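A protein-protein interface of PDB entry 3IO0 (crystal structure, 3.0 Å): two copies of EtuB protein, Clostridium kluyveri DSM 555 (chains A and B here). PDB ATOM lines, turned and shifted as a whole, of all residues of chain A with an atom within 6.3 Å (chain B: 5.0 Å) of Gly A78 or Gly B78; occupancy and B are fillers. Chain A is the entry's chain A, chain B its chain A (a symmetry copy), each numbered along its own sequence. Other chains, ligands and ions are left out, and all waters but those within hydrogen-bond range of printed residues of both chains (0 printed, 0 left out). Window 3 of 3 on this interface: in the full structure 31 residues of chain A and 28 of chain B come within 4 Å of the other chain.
NH2 of Arg A74 sits at hydrogen-bond distance from O of Arg B74 (2.7 Å).
Of the printed residues of chain B, Gly A78 touches Gly B78 (3.998 Å).
Printed residues of chain A within 4 Å of Gly B78: Gly A78 (3.998 Å).
Printed residues of chain A within 4 Å of Asp B75: Arg A74 (3.96 Å).
Printed residues of chain B within 4 Å of Arg A74: Arg B74 and Asp B75.
Gly B79 touches none of the printed residues of chain A.
Ala A80 touches none of the printed residues of chain B.
The nearest printed residue of chain B that does not touch Gly A78 is Lys B77 (4.1 Å).
The nearest printed residue of chain A that does not touch Gly B78 is Gly A79 (4.1 Å).
Arg B74 touches its own counterpart, Arg A74.
Arg A74 touches Asp B75, but with the chains exchanged Asp A75 does not touch Arg B74 (7.1 Å).
Gly A78 touches its own counterpart, Gly B78.
7 positions are printed for both chains.
Of the 3 pairs that touch across the chains among the printed residues, 2 have their exchanged pair printed and touching as well.
Along chain A the printed residues that touch a printed residue of chain B span positions 74 to 78.
Printed residues of chain B that touch a printed residue of chain A: Arg B74, Asp B75 and Gly B78.
Among the printed residues, 3 pairs touch across the chains.
Among the printed residues, no Asp or Glu carboxylate lies within 4 Å of a Lys or Arg side-chain nitrogen of the other chain.
Among the printed residues, pairs that only touch across the chains: Arg A74 with Asp B75 (3.96 Å) and Gly A78 with Gly B78 (3.998 Å).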
ATOM      1  N   ARG A  46      29.331  -7.745  19.177  1.00  0.00           N
ATOM      2  CA  ARG A  46      28.916  -7.877  17.794  1.00  0.00           C
ATOM      3  C   ARG A  46      29.834  -8.841  17.073  1.00  0.00           C
ATOM      4  O   ARG A  46      29.378  -9.620  16.244  1.00  0.00           O
ATOM      5  CB  ARG A  46      28.923  -6.523  17.082  1.00  0.00           C
ATOM      6  CG  ARG A  46      28.030  -5.450  17.723  1.00  0.00           C
ATOM      7  CD  ARG A  46      26.545  -5.774  17.622  1.00  0.00           C
ATOM      8  NE  ARG A  46      26.143  -6.146  16.262  1.00  0.00           N
ATOM      9  CZ  ARG A  46      26.048  -5.309  15.236  1.00  0.00           C
ATOM     10  NH1 ARG A  46      26.332  -4.022  15.384  1.00  0.00           N
ATOM     11  NH2 ARG A  46      25.673  -5.769  14.051  1.00  0.00           N
ATOM     12  N   ARG A  74      25.610 -14.868  15.054  1.00  0.00           N
ATOM     13  CA  ARG A  74      24.968 -14.502  13.783  1.00  0.00           C
ATOM     14  C   ARG A  74      24.965 -13.044  13.573  1.00  0.00           C
ATOM     15  O   ARG A  74      23.940 -12.410  13.330  1.00  0.00           O
ATOM     16  CB  ARG A  74      23.758 -15.252  13.260  1.00  0.00           C
ATOM     17  CG  ARG A  74      23.900 -15.335  11.678  1.00  0.00           C
ATOM     18  CD  ARG A  74      25.319 -15.857  11.238  1.00  0.00           C
ATOM     19  NE  ARG A  74      25.747 -15.594   9.851  1.00  0.00           N
ATOM     20  CZ  ARG A  74      26.780 -14.810   9.504  1.00  0.00           C
ATOM     21  NH1 ARG A  74      27.497 -14.180  10.429  1.00  0.00           N
ATOM     22  NH2 ARG A  74      27.101 -14.629   8.229  1.00  0.00           N
ATOM     23  N   ASP A  75      26.191 -12.548  13.659  1.00  0.00           N
ATOM     24  CA  ASP A  75      26.475 -11.154  13.632  1.00  0.00           C
ATOM     25  C   ASP A  75      27.755 -11.024  12.829  1.00  0.00           C
ATOM     26  O   ASP A  75      27.869 -11.629  11.746  1.00  0.00           O
ATOM     27  CB  ASP A  75      26.660 -10.668  15.056  1.00  0.00           C
ATOM     28  CG  ASP A  75      26.358  -9.209  15.198  1.00  0.00           C
ATOM     29  OD1 ASP A  75      26.519  -8.460  14.203  1.00  0.00           O
ATOM     30  OD2 ASP A  75      25.953  -8.803  16.299  1.00  0.00           O
ATOM     31  N   THR A  76      28.678 -10.201  13.331  1.00  0.00           N
ATOM     32  CA  THR A  76      30.101 -10.336  13.062  1.00  0.00           C
ATOM     33  C   THR A  76      30.694  -9.760  11.789  1.00  0.00           C
ATOM     34  O   THR A  76      31.722 -10.249  11.385  1.00  0.00           O
ATOM     35  CB  THR A  76      30.520 -11.833  13.056  1.00  0.00           C
ATOM     36  OG1 THR A  76      31.871 -11.965  13.497  1.00  0.00           O
ATOM     37  CG2 THR A  76      30.419 -12.413  11.670  1.00  0.00           C
ATOM     38  N   LYS A  77      30.157  -8.739  11.139  1.00  0.00           N
ATOM     39  CA  LYS A  77      29.111  -7.884  11.570  1.00  0.00           C
ATOM     40  C   LYS A  77      28.685  -7.257  10.233  1.00  0.00           C
ATOM     41  O   LYS A  77      28.991  -6.095   9.992  1.00  0.00           O
ATOM     42  CB  LYS A  77      29.739  -6.838  12.488  1.00  0.00           C
ATOM     43  CG  LYS A  77      28.814  -5.834  13.082  1.00  0.00           C
ATOM     44  CD  LYS A  77      29.399  -4.432  12.946  1.00  0.00           C
ATOM     45  CE  LYS A  77      30.266  -4.006  14.121  1.00  0.00           C
ATOM     46  NZ  LYS A  77      30.422  -2.510  14.146  1.00  0.00           N
ATOM     47  N   GLY A  78      28.134  -8.029   9.286  1.00  0.00           N
ATOM     48  CA  GLY A  78      28.338  -9.481   9.128  1.00  0.00           C
ATOM     49  C   GLY A  78      29.037  -9.703   7.790  1.00  0.00           C
ATOM     50  O   GLY A  78      29.424  -8.739   7.183  1.00  0.00           O
ATOM     51  N   GLY A  79      29.265 -10.934   7.321  1.00  0.00           N
ATOM     52  CA  GLY A  79      29.189 -12.195   8.101  1.00  0.00           C
ATOM     53  C   GLY A  79      30.580 -12.265   8.656  1.00  0.00           C
ATOM     54  O   GLY A  79      31.118 -11.213   8.935  1.00  0.00           O
ATOM     55  N   ALA A  80      31.199 -13.436   8.815  1.00  0.00           N
ATOM     56  CA  ALA A  80      30.638 -14.756   8.554  1.00  0.00           C
ATOM     57  C   ALA A  80      30.460 -15.614   9.835  1.00  0.00           C
ATOM     58  O   ALA A  80      30.094 -16.787   9.734  1.00  0.00           O
ATOM     59  CB  ALA A  80      31.536 -15.494   7.560  1.00  0.00           C
ATOM     60  N   ARG B  74      23.522 -18.244   4.808  1.00  0.00           N
ATOM     61  CA  ARG B  74      23.408 -17.171   5.807  1.00  0.00           C
ATOM     62  C   ARG B  74      24.634 -16.358   5.876  1.00  0.00           C
ATOM     63  O   ARG B  74      25.238 -16.154   6.927  1.00  0.00           O
ATOM     64  CB  ARG B  74      22.675 -17.382   7.117  1.00  0.00           C
ATOM     65  CG  ARG B  74      21.924 -16.022   7.463  1.00  0.00           C
ATOM     66  CD  ARG B  74      21.086 -15.483   6.245  1.00  0.00           C
ATOM     67  NE  ARG B  74      20.691 -14.062   6.259  1.00  0.00           N
ATOM     68  CZ  ARG B  74      21.117 -13.139   5.383  1.00  0.00           C
ATOM     69  NH1 ARG B  74      21.974 -13.461   4.419  1.00  0.00           N
ATOM     70  NH2 ARG B  74      20.709 -11.879   5.465  1.00  0.00           N
ATOM     71  N   ASP B  75      24.956 -15.878   4.683  1.00  0.00           N
ATOM     72  CA  ASP B  75      26.162 -15.170   4.423  1.00  0.00           C
ATOM     73  C   ASP B  75      25.778 -14.074   3.448  1.00  0.00           C
ATOM     74  O   ASP B  75      24.768 -13.378   3.668  1.00  0.00           O
ATOM     75  CB  ASP B  75      27.166 -16.129   3.813  1.00  0.00           C
ATOM     76  CG  ASP B  75      28.578 -15.698   4.061  1.00  0.00           C
ATOM     77  OD1 ASP B  75      28.819 -14.475   4.211  1.00  0.00           O
ATOM     78  OD2 ASP B  75      29.454 -16.577   4.112  1.00  0.00           O
ATOM     79  N   THR B  76      26.606 -13.893   2.417  1.00  0.00           N
ATOM     80  CA  THR B  76      26.186 -13.330   1.143  1.00  0.00           C
ATOM     81  C   THR B  76      26.098 -11.825   0.966  1.00  0.00           C
ATOM     82  O   THR B  76      25.356 -11.409   0.109  1.00  0.00           O
ATOM     83  CB  THR B  76      24.781 -13.862   0.744  1.00  0.00           C
ATOM     84  OG1 THR B  76      24.668 -13.926  -0.678  1.00  0.00           O
ATOM     85  CG2 THR B  76      23.697 -12.954   1.261  1.00  0.00           C
ATOM     86  N   LYS B  77      26.818 -10.971   1.677  1.00  0.00           N
ATOM     87  CA  LYS B  77      27.904 -11.255   2.544  1.00  0.00           C
ATOM     88  C   LYS B  77      27.969  -9.953   3.358  1.00  0.00           C
ATOM     89  O   LYS B  77      28.875  -9.156   3.141  1.00  0.00           O
ATOM     90  CB  LYS B  77      29.145 -11.414   1.668  1.00  0.00           C
ATOM     91  CG  LYS B  77      30.416 -11.740   2.370  1.00  0.00           C
ATOM     92  CD  LYS B  77      31.545 -10.853   1.856  1.00  0.00           C
ATOM     93  CE  LYS B  77      32.302 -11.437   0.673  1.00  0.00           C
ATOM     94  NZ  LYS B  77      33.640 -10.764   0.520  1.00  0.00           N
ATOM     95  N   GLY B  78      26.953  -9.628   4.169  1.00  0.00           N
ATOM     96  CA  GLY B  78      25.553 -10.069   4.021  1.00  0.00           C
ATOM     97  C   GLY B  78      24.706  -8.826   3.762  1.00  0.00           C
ATOM     98  O   GLY B  78      25.272  -7.780   3.579  1.00  0.00           O
ATOM     99  N   GLY B  79      23.374  -8.898   3.685  1.00  0.00           N
ATOM    100  CA  GLY B  79      22.573 -10.136   3.519  1.00  0.00           C
ATOM    101  C   GLY B  79      22.558 -10.261   2.024  1.00  0.00           C
ATOM    102  O   GLY B  79      23.550  -9.895   1.429  1.00  0.00           O
ATOM    103  N   ALA B  80      21.487 -10.737   1.384  1.00  0.00           N
ATOM    104  CA  ALA B  80      20.265 -11.242   1.996  1.00  0.00           C
ATOM    105  C   ALA B  80      20.047 -12.763   1.774  1.00  0.00           C
ATOM    106  O   ALA B  80      18.998 -13.287   2.152  1.00  0.00           O
ATOM    107  CB  ALA B  80      19.070 -10.465   1.442  1.00  0.00           C
